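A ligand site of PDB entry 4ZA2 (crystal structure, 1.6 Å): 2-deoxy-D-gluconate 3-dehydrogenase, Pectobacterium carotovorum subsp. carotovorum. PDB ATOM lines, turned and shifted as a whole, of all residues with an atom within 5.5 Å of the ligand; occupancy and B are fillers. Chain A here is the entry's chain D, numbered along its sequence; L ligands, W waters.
OH of Tyr 158 lies within hydrogen-bond range of O13 of the ligand.
The backbone carbonyl oxygen (O) of Gly 189 is in hydrogen-bond range of a nitrogen (N7) of the ligand (3.4 Å).
OD1 of Asp 19 sits at hydrogen-bond distance from O5 of the ligand (2.5 Å).
The backbone NH (N) of Asn 195 lies close to an oxygen (O7) of the ligand, at 3.5 Å.
An oxygen (O5) of the ligand sits at hydrogen-bond distance from the backbone carbonyl oxygen of Gly 17 (3.3 Å).
N3 of the ligand lies within hydrogen-bond range of OD1 of Asp 65, 2.7 Å away.
An oxygen (O12) of the ligand sits at hydrogen-bond distance from the side-chain amino group (NZ) of Lys 162, at 3.1 Å.
N of Met 66 sits at hydrogen-bond distance from N4 of the ligand, at 3.0 Å.
The side-chain hydroxyl (OG1) of Thr 193 lies within hydrogen-bond range of an oxygen (O8) of the ligand, 2.6 Å away.
The backbone carbonyl oxygen (O) of Asn 92 sits at hydrogen-bond distance from an oxygen (O12) of the ligand.
The backbone NH (N) of Leu 22 lies within hydrogen-bond range of an oxygen (O9) of the ligand (3.2 Å).
An oxygen (O4) of the ligand lies within hydrogen-bond range of the backbone NH (N) of Gly 94 (3.5 Å).
The backbone NH of Ala 93 lies within hydrogen-bond range of the side-chain hydroxyl of Thr 16.
The backbone carbonyl oxygen of Met 191 is in hydrogen-bond range of the side-chain hydroxyl of Thr 196, 2.7 Å away.
N of Asn 92 sits at hydrogen-bond distance from OG1 of Thr 16.
N of Asn 195 sits close to OG1 of Thr 193 (3.5 Å).
SD of Met 191 sits at hydrogen-bond distance from N of Gly 189 (3.6 Å).
The side-chain hydroxyl of Thr 196 is in hydrogen-bond range of the backbone carbonyl oxygen of Thr 193, at 3.2 Å.
NZ of Lys 162 is in hydrogen-bond range of O of Ile 143, at 2.9 Å.
The side-chain amide nitrogen (ND2) of Asn 92 sits at hydrogen-bond distance from the backbone carbonyl oxygen (O) of Gly 17, 2.8 Å away.
The backbone NH (N) of Met 191 sits close to a nitrogen (N7) of the ligand (3.1 Å).
Merely in contact with the ligand: Ala 144, Thr 196, Ala 93, Ile 42, Leu 115, Thr 20, Ile 143, Ser 145, Ala 64, Pro 188, Asn 194, Ile 95, Gly 21 and Tyr 190.
Hydrophobic or aromatic side chains within 4 Å of the ligand: Leu 22, Ile 42, Met 66, Ala 93, Ile 95, Leu 115, Ile 143, Tyr 158, Pro 188 and Met 191.
Within 4 Å of the ligand: Gly 17, Asp 19, Thr 20, Gly 21, Leu 22, Ile 42, Ala 64, Asp 65, Met 66, Asn 92, Ala 93, Gly 94, Ile 95, Leu 115, Ile 143, Ala 144, Ser 145, Tyr 158, Lys 162, Pro 188, Gly 189, Tyr 190, Met 191, Thr 193, Asn 194, Asn 195 and Thr 196.
The nearest printed residue that does not touch the ligand is Cys 18 (4.02 Å).
Water W1 lies within hydrogen-bond range of an oxygen (O6) of the ligand, the backbone NH (N) of Ile 42, the side-chain carboxylate (OD1) of Asp 19 and the side-chain amide oxygen (OD1) of Asn 41.
Water W3 lies within hydrogen-bond range of an oxygen (O1) of the ligand (2.8 Å), the side-chain amide oxygen (OD1) of Asn 195 (2.9 Å) and the backbone carbonyl oxygen (O) of Gly 94 (3.0 Å).
Water W2 lies within hydrogen-bond range of the backbone NH of Asn 194 (2.9 Å) and an oxygen (O2) of the ligand (2.9 Å).
Water W4 lies within hydrogen-bond range of O of Pro 188 (2.8 Å), N of Met 146 (3.0 Å), OG of Ser 145 (3.2 Å) and O of Gly 189 (3.2 Å).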
ATOM      1  N   THR A  16     -27.877   8.274 -25.942  1.00  0.00           N
ATOM      2  CA  THR A  16     -26.619   7.803 -26.518  1.00  0.00           C
ATOM      3  C   THR A  16     -25.548   7.631 -25.434  1.00  0.00           C
ATOM      4  O   THR A  16     -25.420   8.477 -24.541  1.00  0.00           O
ATOM      5  CB  THR A  16     -26.109   8.760 -27.619  1.00  0.00           C
ATOM      6  OG1 THR A  16     -25.657   9.987 -27.030  1.00  0.00           O
ATOM      7  CG2 THR A  16     -27.216   9.056 -28.621  1.00  0.00           C
ATOM      8  N   GLY A  17     -24.788   6.558 -25.510  1.00  0.00           N
ATOM      9  CA  GLY A  17     -23.770   6.241 -24.512  1.00  0.00           C
ATOM     10  C   GLY A  17     -24.336   5.976 -23.119  1.00  0.00           C
ATOM     11  O   GLY A  17     -24.008   6.686 -22.174  1.00  0.00           O
ATOM     12  N   CYS A  18     -25.163   4.934 -22.995  1.00  0.00           N
ATOM     13  CA  CYS A  18     -25.800   4.628 -21.703  1.00  0.00           C
ATOM     14  C   CYS A  18     -25.436   3.239 -21.169  1.00  0.00           C
ATOM     15  O   CYS A  18     -26.185   2.673 -20.384  1.00  0.00           O
ATOM     16  CB  CYS A  18     -27.319   4.790 -21.827  1.00  0.00           C
ATOM     17  SG  CYS A  18     -28.052   3.765 -23.129  1.00  0.00           S
ATOM     18  N   ASP A  19     -24.282   2.722 -21.576  1.00  0.00           N
ATOM     19  CA  ASP A  19     -23.816   1.425 -21.079  1.00  0.00           C
ATOM     20  C   ASP A  19     -23.235   1.528 -19.666  1.00  0.00           C
ATOM     21  O   ASP A  19     -23.177   0.518 -18.959  1.00  0.00           O
ATOM     22  CB  ASP A  19     -22.793   0.806 -22.045  1.00  0.00           C
ATOM     23  CG  ASP A  19     -21.480   1.568 -22.078  1.00  0.00           C
ATOM     24  OD1 ASP A  19     -21.420   2.612 -22.749  1.00  0.00           O
ATOM     25  OD2 ASP A  19     -20.504   1.113 -21.441  1.00  0.00           O
ATOM     26  N   THR A  20     -22.822   2.723 -19.272  1.00  0.00           N
ATOM     27  CA  THR A  20     -22.146   2.932 -17.990  1.00  0.00           C
ATOM     28  C   THR A  20     -22.270   4.387 -17.513  1.00  0.00           C
ATOM     29  O   THR A  20     -22.781   5.244 -18.236  1.00  0.00           O
ATOM     30  CB  THR A  20     -20.652   2.565 -18.100  1.00  0.00           C
ATOM     31  OG1 THR A  20     -20.037   2.627 -16.807  1.00  0.00           O
ATOM     32  CG2 THR A  20     -19.924   3.508 -19.062  1.00  0.00           C
ATOM     33  N   GLY A  21     -21.833   4.643 -16.284  1.00  0.00           N
ATOM     34  CA  GLY A  21     -21.671   6.017 -15.775  1.00  0.00           C
ATOM     35  C   GLY A  21     -22.911   6.885 -15.826  1.00  0.00           C
ATOM     36  O   GLY A  21     -23.999   6.451 -15.449  1.00  0.00           O
ATOM     37  N   LEU A  22     -22.742   8.115 -16.306  1.00  0.00           N
ATOM     38  CA  LEU A  22     -23.815   9.094 -16.290  1.00  0.00           C
ATOM     39  C   LEU A  22     -24.989   8.702 -17.186  1.00  0.00           C
ATOM     40  O   LEU A  22     -26.139   8.848 -16.796  1.00  0.00           O
ATOM     41  CB  LEU A  22     -23.302  10.480 -16.693  1.00  0.00           C
ATOM     42  CG  LEU A  22     -22.184  11.058 -15.820  1.00  0.00           C
ATOM     43  CD1 LEU A  22     -21.847  12.475 -16.292  1.00  0.00           C
ATOM     44  CD2 LEU A  22     -22.561  11.065 -14.350  1.00  0.00           C
ATOM     45  N   GLY A  23     -24.689   8.204 -18.389  1.00  0.00           N
ATOM     46  CA  GLY A  23     -25.722   7.861 -19.350  1.00  0.00           C
ATOM     47  C   GLY A  23     -26.615   6.727 -18.855  1.00  0.00           C
ATOM     48  O   GLY A  23     -27.821   6.740 -19.051  1.00  0.00           O
ATOM     49  N   VAL A  40     -28.041   3.781 -27.815  1.00  0.00           N
ATOM     50  CA  VAL A  40     -27.082   3.758 -28.925  1.00  0.00           C
ATOM     51  C   VAL A  40     -25.684   3.750 -28.313  1.00  0.00           C
ATOM     52  O   VAL A  40     -25.298   4.701 -27.627  1.00  0.00           O
ATOM     53  CB  VAL A  40     -27.243   4.962 -29.873  1.00  0.00           C
ATOM     54  CG1 VAL A  40     -26.327   4.821 -31.085  1.00  0.00           C
ATOM     55  CG2 VAL A  40     -28.695   5.115 -30.307  1.00  0.00           C
ATOM     56  N   ASN A  41     -24.933   2.671 -28.553  1.00  0.00           N
ATOM     57  CA  ASN A  41     -23.666   2.437 -27.851  1.00  0.00           C
ATOM     58  C   ASN A  41     -22.576   1.796 -28.718  1.00  0.00           C
ATOM     59  O   ASN A  41     -22.857   1.307 -29.812  1.00  0.00           O
ATOM     60  CB  ASN A  41     -23.914   1.553 -26.643  1.00  0.00           C
ATOM     61  CG  ASN A  41     -24.726   2.247 -25.566  1.00  0.00           C
ATOM     62  OD1 ASN A  41     -24.199   3.067 -24.803  1.00  0.00           O
ATOM     63  ND2 ASN A  41     -26.017   1.925 -25.488  1.00  0.00           N
ATOM     64  N   ILE A  42     -21.349   1.815 -28.207  1.00  0.00           N
ATOM     65  CA  ILE A  42     -20.210   1.112 -28.811  1.00  0.00           C
ATOM     66  C   ILE A  42     -20.074  -0.300 -28.232  1.00  0.00           C
ATOM     67  O   ILE A  42     -19.564  -1.209 -28.890  1.00  0.00           O
ATOM     68  CB  ILE A  42     -18.877   1.867 -28.568  1.00  0.00           C
ATOM     69  CG1 ILE A  42     -18.890   3.230 -29.271  1.00  0.00           C
ATOM     70  CG2 ILE A  42     -17.677   1.046 -29.010  1.00  0.00           C
ATOM     71  CD1 ILE A  42     -18.940   3.150 -30.782  1.00  0.00           C
ATOM     72  N   VAL A  43     -20.502  -0.471 -26.980  1.00  0.00           N
ATOM     73  CA  VAL A  43     -20.494  -1.781 -26.333  1.00  0.00           C
ATOM     74  C   VAL A  43     -21.896  -2.095 -25.818  1.00  0.00           C
ATOM     75  O   VAL A  43     -22.681  -1.181 -25.553  1.00  0.00           O
ATOM     76  CB  VAL A  43     -19.480  -1.852 -25.170  1.00  0.00           C
ATOM     77  CG1 VAL A  43     -18.053  -1.837 -25.716  1.00  0.00           C
ATOM     78  CG2 VAL A  43     -19.680  -0.713 -24.172  1.00  0.00           C
ATOM     79  N   ALA A  64     -23.732   1.501 -32.736  1.00  0.00           N
ATOM     80  CA  ALA A  64     -23.187   2.365 -33.786  1.00  0.00           C
ATOM     81  C   ALA A  64     -22.141   3.355 -33.235  1.00  0.00           C
ATOM     82  O   ALA A  64     -22.193   3.728 -32.068  1.00  0.00           O
ATOM     83  CB  ALA A  64     -24.306   3.139 -34.467  1.00  0.00           C
ATOM     84  N   ASP A  65     -21.202   3.754 -34.089  1.00  0.00           N
ATOM     85  CA  ASP A  65     -20.299   4.869 -33.803  1.00  0.00           C
ATOM     86  C   ASP A  65     -21.071   6.165 -34.058  1.00  0.00           C
ATOM     87  O   ASP A  65     -21.403   6.479 -35.205  1.00  0.00           O
ATOM     88  CB  ASP A  65     -19.042   4.809 -34.679  1.00  0.00           C
ATOM     89  CG  ASP A  65     -18.087   5.975 -34.433  1.00  0.00           C
ATOM     90  OD1 ASP A  65     -18.268   6.710 -33.433  1.00  0.00           O
ATOM     91  OD2 ASP A  65     -17.149   6.165 -35.235  1.00  0.00           O
ATOM     92  N   MET A  66     -21.365   6.910 -32.985  1.00  0.00           N
ATOM     93  CA  MET A  66     -22.202   8.100 -33.076  1.00  0.00           C
ATOM     94  C   MET A  66     -21.564   9.193 -33.933  1.00  0.00           C
ATOM     95  O   MET A  66     -22.279  10.039 -34.473  1.00  0.00           O
ATOM     96  CB  MET A  66     -22.552   8.651 -31.676  1.00  0.00           C
ATOM     97  CG  MET A  66     -23.770   8.014 -31.024  1.00  0.00           C
ATOM     98  SD  MET A  66     -25.334   8.273 -31.906  1.00  0.00           S
ATOM     99  CE  MET A  66     -25.319  10.050 -32.136  1.00  0.00           C
ATOM    100  N   SER A  67     -20.238   9.158 -34.070  1.00  0.00           N
ATOM    101  CA  SER A  67     -19.508  10.096 -34.918  1.00  0.00           C
ATOM    102  C   SER A  67     -19.830   9.980 -36.412  1.00  0.00           C
ATOM    103  O   SER A  67     -19.610  10.932 -37.161  1.00  0.00           O
ATOM    104  CB  SER A  67     -18.002   9.946 -34.708  1.00  0.00           C
ATOM    105  OG  SER A  67     -17.645  10.336 -33.396  1.00  0.00           O
ATOM    106  N   ASN A  91     -28.156  13.516 -25.561  1.00  0.00           N
ATOM    107  CA  ASN A  91     -26.905  13.466 -26.302  1.00  0.00           C
ATOM    108  C   ASN A  91     -25.696  13.316 -25.373  1.00  0.00           C
ATOM    109  O   ASN A  91     -24.933  14.262 -25.177  1.00  0.00           O
ATOM    110  CB  ASN A  91     -26.768  14.706 -27.201  1.00  0.00           C
ATOM    111  CG  ASN A  91     -27.715  14.688 -28.384  1.00  0.00           C
ATOM    112  OD1 ASN A  91     -27.704  13.749 -29.172  1.00  0.00           O
ATOM    113  ND2 ASN A  91     -28.525  15.720 -28.520  1.00  0.00           N
ATOM    114  N   ASN A  92     -25.532  12.120 -24.802  1.00  0.00           N
ATOM    115  CA  ASN A  92     -24.538  11.897 -23.743  1.00  0.00           C
ATOM    116  C   ASN A  92     -23.226  11.267 -24.215  1.00  0.00           C
ATOM    117  O   ASN A  92     -22.178  11.458 -23.597  1.00  0.00           O
ATOM    118  CB  ASN A  92     -25.159  11.068 -22.614  1.00  0.00           C
ATOM    119  CG  ASN A  92     -24.147  10.669 -21.554  1.00  0.00           C
ATOM    120  OD1 ASN A  92     -23.764  11.475 -20.706  1.00  0.00           O
ATOM    121  ND2 ASN A  92     -23.712   9.421 -21.595  1.00  0.00           N
ATOM    122  N   ALA A  93     -23.273  10.527 -25.318  1.00  0.00           N
ATOM    123  CA  ALA A  93     -22.067   9.913 -25.845  1.00  0.00           C
ATOM    124  C   ALA A  93     -20.991  10.973 -26.102  1.00  0.00           C
ATOM    125  O   ALA A  93     -21.236  11.945 -26.827  1.00  0.00           O
ATOM    126  CB  ALA A  93     -22.387   9.165 -27.132  1.00  0.00           C
ATOM    127  N   GLY A  94     -19.825  10.782 -25.491  1.00  0.00           N
ATOM    128  CA  GLY A  94     -18.699  11.696 -25.655  1.00  0.00           C
ATOM    129  C   GLY A  94     -17.381  11.101 -25.192  1.00  0.00           C
ATOM    130  O   GLY A  94     -17.357  10.063 -24.535  1.00  0.00           O
ATOM    131  N   ILE A  95     -16.286  11.779 -25.543  1.00  0.00           N
ATOM    132  CA  ILE A  95     -14.951  11.380 -25.136  1.00  0.00           C
ATOM    133  C   ILE A  95     -14.115  12.590 -24.726  1.00  0.00           C
ATOM    134  O   ILE A  95     -14.518  13.729 -24.933  1.00  0.00           O
ATOM    135  CB  ILE A  95     -14.209  10.633 -26.261  1.00  0.00           C
ATOM    136  CG1 ILE A  95     -14.209  11.469 -27.552  1.00  0.00           C
ATOM    137  CG2 ILE A  95     -14.850   9.278 -26.534  1.00  0.00           C
ATOM    138  CD1 ILE A  95     -13.194  11.017 -28.562  1.00  0.00           C
ATOM    139  N   LEU A 115     -17.394  13.715 -32.159  1.00  0.00           N
ATOM    140  CA  LEU A 115     -18.383  13.129 -31.262  1.00  0.00           C
ATOM    141  C   LEU A 115     -19.067  14.176 -30.381  1.00  0.00           C
ATOM    142  O   LEU A 115     -20.297  14.267 -30.360  1.00  0.00           O
ATOM    143  CB  LEU A 115     -17.727  12.068 -30.383  1.00  0.00           C
ATOM    144  CG  LEU A 115     -18.635  11.211 -29.493  1.00  0.00           C
ATOM    145  CD1 LEU A 115     -19.672  10.453 -30.298  1.00  0.00           C
ATOM    146  CD2 LEU A 115     -17.767  10.269 -28.695  1.00  0.00           C
ATOM    147  N   ASN A 116     -18.273  14.971 -29.669  1.00  0.00           N
ATOM    148  CA  ASN A 116     -18.798  15.838 -28.606  1.00  0.00           C
ATOM    149  C   ASN A 116     -19.650  17.019 -29.088  1.00  0.00           C
ATOM    150  O   ASN A 116     -20.507  17.478 -28.351  1.00  0.00           O
ATOM    151  CB  ASN A 116     -17.664  16.354 -27.721  1.00  0.00           C
ATOM    152  CG  ASN A 116     -17.056  15.274 -26.857  1.00  0.00           C
ATOM    153  OD1 ASN A 116     -17.228  14.079 -27.131  1.00  0.00           O
ATOM    154  ND2 ASN A 116     -16.335  15.675 -25.815  1.00  0.00           N
ATOM    155  N   ILE A 143     -25.429  17.382 -23.028  1.00  0.00           N
ATOM    156  CA  ILE A 143     -24.602  17.283 -21.852  1.00  0.00           C
ATOM    157  C   ILE A 143     -23.434  18.258 -22.012  1.00  0.00           C
ATOM    158  O   ILE A 143     -22.546  18.079 -22.836  1.00  0.00           O
ATOM    159  CB  ILE A 143     -24.139  15.824 -21.609  1.00  0.00           C
ATOM    160  CG1 ILE A 143     -25.351  14.871 -21.575  1.00  0.00           C
ATOM    161  CG2 ILE A 143     -23.316  15.725 -20.317  1.00  0.00           C
ATOM    162  CD1 ILE A 143     -26.353  15.153 -20.478  1.00  0.00           C
ATOM    163  N   ALA A 144     -23.484  19.336 -21.227  1.00  0.00           N
ATOM    164  CA  ALA A 144     -22.420  20.318 -21.181  1.00  0.00           C
ATOM    165  C   ALA A 144     -21.377  19.884 -20.147  1.00  0.00           C
ATOM    166  O   ALA A 144     -21.215  18.684 -19.919  1.00  0.00           O
ATOM    167  CB  ALA A 144     -22.999  21.680 -20.871  1.00  0.00           C
ATOM    168  N   SER A 145     -20.681  20.829 -19.516  1.00  0.00           N
ATOM    169  CA  SER A 145     -19.577  20.525 -18.626  1.00  0.00           C
ATOM    170  C   SER A 145     -19.247  21.765 -17.817  1.00  0.00           C
ATOM    171  O   SER A 145     -19.657  22.870 -18.186  1.00  0.00           O
ATOM    172  CB  SER A 145     -18.351  20.103 -19.459  1.00  0.00           C
ATOM    173  OG  SER A 145     -17.195  19.866 -18.684  1.00  0.00           O
ATOM    174  N   MET A 146     -18.463  21.596 -16.758  1.00  0.00           N
ATOM    175  CA  MET A 146     -17.821  22.745 -16.089  1.00  0.00           C
ATOM    176  C   MET A 146     -16.924  23.464 -17.098  1.00  0.00           C
ATOM    177  O   MET A 146     -16.758  24.699 -17.045  1.00  0.00           O
ATOM    178  CB  MET A 146     -17.037  22.297 -14.857  1.00  0.00           C
ATOM    179  CG  MET A 146     -17.903  21.687 -13.763  1.00  0.00           C
ATOM    180  SD  MET A 146     -19.117  22.783 -13.052  1.00  0.00           S
ATOM    181  CE  MET A 146     -20.560  22.426 -14.033  1.00  0.00           C
ATOM    182  N   TYR A 158     -11.994  19.244 -25.851  1.00  0.00           N
ATOM    183  CA  TYR A 158     -13.091  19.015 -24.918  1.00  0.00           C
ATOM    184  C   TYR A 158     -13.720  20.345 -24.507  1.00  0.00           C
ATOM    185  O   TYR A 158     -14.941  20.509 -24.568  1.00  0.00           O
ATOM    186  CB  TYR A 158     -12.605  18.265 -23.687  1.00  0.00           C
ATOM    187  CG  TYR A 158     -13.705  17.726 -22.806  1.00  0.00           C
ATOM    188  CD1 TYR A 158     -14.297  16.483 -23.063  1.00  0.00           C
ATOM    189  CD2 TYR A 158     -14.146  18.453 -21.712  1.00  0.00           C
ATOM    190  CE1 TYR A 158     -15.310  15.996 -22.253  1.00  0.00           C
ATOM    191  CE2 TYR A 158     -15.159  17.966 -20.902  1.00  0.00           C
ATOM    192  CZ  TYR A 158     -15.738  16.744 -21.185  1.00  0.00           C
ATOM    193  OH  TYR A 158     -16.735  16.310 -20.333  1.00  0.00           O
ATOM    194  N   LYS A 162     -17.512  21.296 -25.533  1.00  0.00           N
ATOM    195  CA  LYS A 162     -18.485  21.494 -24.458  1.00  0.00           C
ATOM    196  C   LYS A 162     -18.978  22.953 -24.368  1.00  0.00           C
ATOM    197  O   LYS A 162     -20.114  23.212 -24.004  1.00  0.00           O
ATOM    198  CB  LYS A 162     -17.910  21.006 -23.142  1.00  0.00           C
ATOM    199  CG  LYS A 162     -17.687  19.500 -23.078  1.00  0.00           C
ATOM    200  CD  LYS A 162     -18.997  18.743 -23.265  1.00  0.00           C
ATOM    201  CE  LYS A 162     -18.838  17.263 -22.957  1.00  0.00           C
ATOM    202  NZ  LYS A 162     -20.102  16.547 -23.233  1.00  0.00           N
ATOM    203  N   PRO A 188     -22.775  18.541 -15.863  1.00  0.00           N
ATOM    204  CA  PRO A 188     -22.335  17.834 -14.655  1.00  0.00           C
ATOM    205  C   PRO A 188     -21.093  18.479 -14.084  1.00  0.00           C
ATOM    206  O   PRO A 188     -20.292  19.052 -14.843  1.00  0.00           O
ATOM    207  CB  PRO A 188     -22.021  16.434 -15.179  1.00  0.00           C
ATOM    208  CG  PRO A 188     -22.764  16.314 -16.441  1.00  0.00           C
ATOM    209  CD  PRO A 188     -22.659  17.680 -17.041  1.00  0.00           C
ATOM    210  N   GLY A 189     -20.925  18.384 -12.766  1.00  0.00           N
ATOM    211  CA  GLY A 189     -19.710  18.836 -12.075  1.00  0.00           C
ATOM    212  C   GLY A 189     -18.665  17.741 -12.187  1.00  0.00           C
ATOM    213  O   GLY A 189     -18.566  17.089 -13.225  1.00  0.00           O
ATOM    214  N   TYR A 190     -17.893  17.528 -11.130  1.00  0.00           N
ATOM    215  CA  TYR A 190     -16.907  16.445 -11.112  1.00  0.00           C
ATOM    216  C   TYR A 190     -17.601  15.186 -10.618  1.00  0.00           C
ATOM    217  O   TYR A 190     -17.883  15.043  -9.441  1.00  0.00           O
ATOM    218  CB  TYR A 190     -15.726  16.782 -10.202  1.00  0.00           C
ATOM    219  CG  TYR A 190     -14.722  17.732 -10.814  1.00  0.00           C
ATOM    220  CD1 TYR A 190     -13.733  17.261 -11.659  1.00  0.00           C
ATOM    221  CD2 TYR A 190     -14.769  19.092 -10.548  1.00  0.00           C
ATOM    222  CE1 TYR A 190     -12.809  18.128 -12.231  1.00  0.00           C
ATOM    223  CE2 TYR A 190     -13.852  19.966 -11.118  1.00  0.00           C
ATOM    224  CZ  TYR A 190     -12.871  19.468 -11.948  1.00  0.00           C
ATOM    225  OH  TYR A 190     -11.961  20.319 -12.524  1.00  0.00           O
ATOM    226  N   MET A 191     -17.896  14.301 -11.565  1.00  0.00           N
ATOM    227  CA  MET A 191     -18.649  13.069 -11.298  1.00  0.00           C
ATOM    228  C   MET A 191     -17.723  11.845 -11.291  1.00  0.00           C
ATOM    229  O   MET A 191     -16.778  11.753 -12.077  1.00  0.00           O
ATOM    230  CB  MET A 191     -19.721  12.858 -12.365  1.00  0.00           C
ATOM    231  CG  MET A 191     -20.475  14.127 -12.821  1.00  0.00           C
ATOM    232  SD  MET A 191     -21.311  15.050 -11.520  1.00  0.00           S
ATOM    233  CE  MET A 191     -22.863  14.154 -11.396  1.00  0.00           C
ATOM    234  N   ALA A 192     -18.035  10.888 -10.423  1.00  0.00           N
ATOM    235  CA  ALA A 192     -17.257   9.644 -10.320  1.00  0.00           C
ATOM    236  C   ALA A 192     -17.642   8.682 -11.443  1.00  0.00           C
ATOM    237  O   ALA A 192     -18.605   7.913 -11.319  1.00  0.00           O
ATOM    238  CB  ALA A 192     -17.476   9.001  -8.956  1.00  0.00           C
ATOM    239  N   THR A 193     -16.895   8.735 -12.533  1.00  0.00           N
ATOM    240  CA  THR A 193     -17.146   7.873 -13.703  1.00  0.00           C
ATOM    241  C   THR A 193     -15.800   7.512 -14.335  1.00  0.00           C
ATOM    242  O   THR A 193     -14.745   7.955 -13.870  1.00  0.00           O
ATOM    243  CB  THR A 193     -18.054   8.566 -14.748  1.00  0.00           C
ATOM    244  OG1 THR A 193     -17.421   9.757 -15.238  1.00  0.00           O
ATOM    245  CG2 THR A 193     -19.408   8.939 -14.146  1.00  0.00           C
ATOM    246  N   ASN A 194     -15.841   6.711 -15.403  1.00  0.00           N
ATOM    247  CA  ASN A 194     -14.621   6.353 -16.136  1.00  0.00           C
ATOM    248  C   ASN A 194     -13.902   7.590 -16.676  1.00  0.00           C
ATOM    249  O   ASN A 194     -12.678   7.614 -16.770  1.00  0.00           O
ATOM    250  CB  ASN A 194     -14.923   5.382 -17.282  1.00  0.00           C
ATOM    251  CG  ASN A 194     -15.328   4.005 -16.784  1.00  0.00           C
ATOM    252  OD1 ASN A 194     -15.087   3.648 -15.628  1.00  0.00           O
ATOM    253  ND2 ASN A 194     -15.963   3.225 -17.657  1.00  0.00           N
ATOM    254  N   ASN A 195     -14.666   8.625 -17.012  1.00  0.00           N
ATOM    255  CA  ASN A 195     -14.125   9.894 -17.495  1.00  0.00           C
ATOM    256  C   ASN A 195     -13.120  10.555 -16.537  1.00  0.00           C
ATOM    257  O   ASN A 195     -12.219  11.265 -16.993  1.00  0.00           O
ATOM    258  CB  ASN A 195     -15.263  10.880 -17.785  1.00  0.00           C
ATOM    259  CG  ASN A 195     -14.900  11.907 -18.841  1.00  0.00           C
ATOM    260  OD1 ASN A 195     -14.335  11.564 -19.883  1.00  0.00           O
ATOM    261  ND2 ASN A 195     -15.238  13.171 -18.588  1.00  0.00           N
ATOM    262  N   THR A 196     -13.288  10.331 -15.237  1.00  0.00           N
ATOM    263  CA  THR A 196     -12.454  10.982 -14.209  1.00  0.00           C
ATOM    264  C   THR A 196     -11.603  10.003 -13.402  1.00  0.00           C
ATOM    265  O   THR A 196     -11.302  10.257 -12.239  1.00  0.00           O
ATOM    266  CB  THR A 196     -13.343  11.777 -13.225  1.00  0.00           C
ATOM    267  OG1 THR A 196     -14.324  10.905 -12.648  1.00  0.00           O
ATOM    268  CG2 THR A 196     -14.030  12.919 -13.938  1.00  0.00           C
HETATM  269  P1  LIG L   1     -17.811   7.741 -20.022  1.00  0.00           P
HETATM  270  O1  LIG L   1     -16.566   7.875 -20.872  1.00  0.00           O
HETATM  271  O2  LIG L   1     -17.874   6.325 -19.470  1.00  0.00           O
HETATM  272  O3  LIG L   1     -19.167   8.042 -20.862  1.00  0.00           O
HETATM  273  C1  LIG L   1     -18.962   8.060 -22.286  1.00  0.00           C
HETATM  274  C2  LIG L   1     -20.104   7.270 -22.924  1.00  0.00           C
HETATM  275  O4  LIG L   1     -20.134   7.511 -24.346  1.00  0.00           O
HETATM  276  C3  LIG L   1     -19.902   5.757 -22.728  1.00  0.00           C
HETATM  277  O5  LIG L   1     -21.165   5.092 -22.603  1.00  0.00           O
HETATM  278  C4  LIG L   1     -19.135   5.391 -24.022  1.00  0.00           C
HETATM  279  O6  LIG L   1     -19.190   4.010 -24.362  1.00  0.00           O
HETATM  280  C5  LIG L   1     -19.920   6.261 -25.035  1.00  0.00           C
HETATM  281  N1  LIG L   1     -19.210   6.476 -26.296  1.00  0.00           N
HETATM  282  C6  LIG L   1     -17.892   6.802 -26.456  1.00  0.00           C
HETATM  283  N2  LIG L   1     -17.613   6.902 -27.732  1.00  0.00           N
HETATM  284  C7  LIG L   1     -18.730   6.656 -28.450  1.00  0.00           C
HETATM  285  C8  LIG L   1     -19.048   6.627 -29.829  1.00  0.00           C
HETATM  286  N3  LIG L   1     -18.057   6.889 -30.767  1.00  0.00           N
HETATM  287  N4  LIG L   1     -20.297   6.338 -30.192  1.00  0.00           N
HETATM  288  C9  LIG L   1     -21.235   6.084 -29.301  1.00  0.00           C
HETATM  289  N5  LIG L   1     -20.999   6.100 -28.003  1.00  0.00           N
HETATM  290  C10 LIG L   1     -19.765   6.380 -27.540  1.00  0.00           C
HETATM  291  O7  LIG L   1     -17.681   8.769 -18.771  1.00  0.00           O
HETATM  292  P2  LIG L   1     -19.013   9.665 -18.518  1.00  0.00           P
HETATM  293  O8  LIG L   1     -18.724  10.596 -17.324  1.00  0.00           O
HETATM  294  O9  LIG L   1     -20.203   8.754 -18.140  1.00  0.00           O
HETATM  295  O10 LIG L   1     -19.278  10.562 -19.846  1.00  0.00           O
HETATM  296  C11 LIG L   1     -20.664  10.850 -20.071  1.00  0.00           C
HETATM  297  C12 LIG L   1     -20.847  12.238 -20.718  1.00  0.00           C
HETATM  298  O11 LIG L   1     -20.843  13.247 -19.681  1.00  0.00           O
HETATM  299  C13 LIG L   1     -19.739  12.632 -21.733  1.00  0.00           C
HETATM  300  O12 LIG L   1     -20.262  13.456 -22.794  1.00  0.00           O
HETATM  301  C14 LIG L   1     -18.775  13.407 -20.816  1.00  0.00           C
HETATM  302  O13 LIG L   1     -17.856  14.203 -21.577  1.00  0.00           O
HETATM  303  C15 LIG L   1     -19.822  14.218 -20.019  1.00  0.00           C
HETATM  304  N6  LIG L   1     -19.300  14.857 -18.798  1.00  0.00           N
HETATM  305  C16 LIG L   1     -18.792  14.111 -17.824  1.00  0.00           C
HETATM  306  C17 LIG L   1     -18.300  14.695 -16.642  1.00  0.00           C
HETATM  307  C18 LIG L   1     -17.724  13.863 -15.554  1.00  0.00           C
HETATM  308  O14 LIG L   1     -17.879  12.662 -15.560  1.00  0.00           O
HETATM  309  N7  LIG L   1     -17.000  14.411 -14.547  1.00  0.00           N
HETATM  310  C19 LIG L   1     -18.366  16.099 -16.541  1.00  0.00           C
HETATM  311  C20 LIG L   1     -18.907  16.838 -17.578  1.00  0.00           C
HETATM  312  C21 LIG L   1     -19.372  16.181 -18.709  1.00  0.00           C
HETATM  313  O   HOH W   1     -21.057   2.803 -25.570  1.00  0.00           O
HETATM  314  O   HOH W   2     -18.238   5.819 -16.671  1.00  0.00           O
HETATM  315  O   HOH W   3     -15.765  10.299 -21.999  1.00  0.00           O
HETATM  316  O   HOH W   4     -17.605  18.954 -15.645  1.00  0.00           O
HETATM  317  O   HOH W   5     -22.106   7.757 -19.660  1.00  0.00           O
HETATM  318  O   HOH W   6     -22.133  14.135 -25.539  1.00  0.00           O
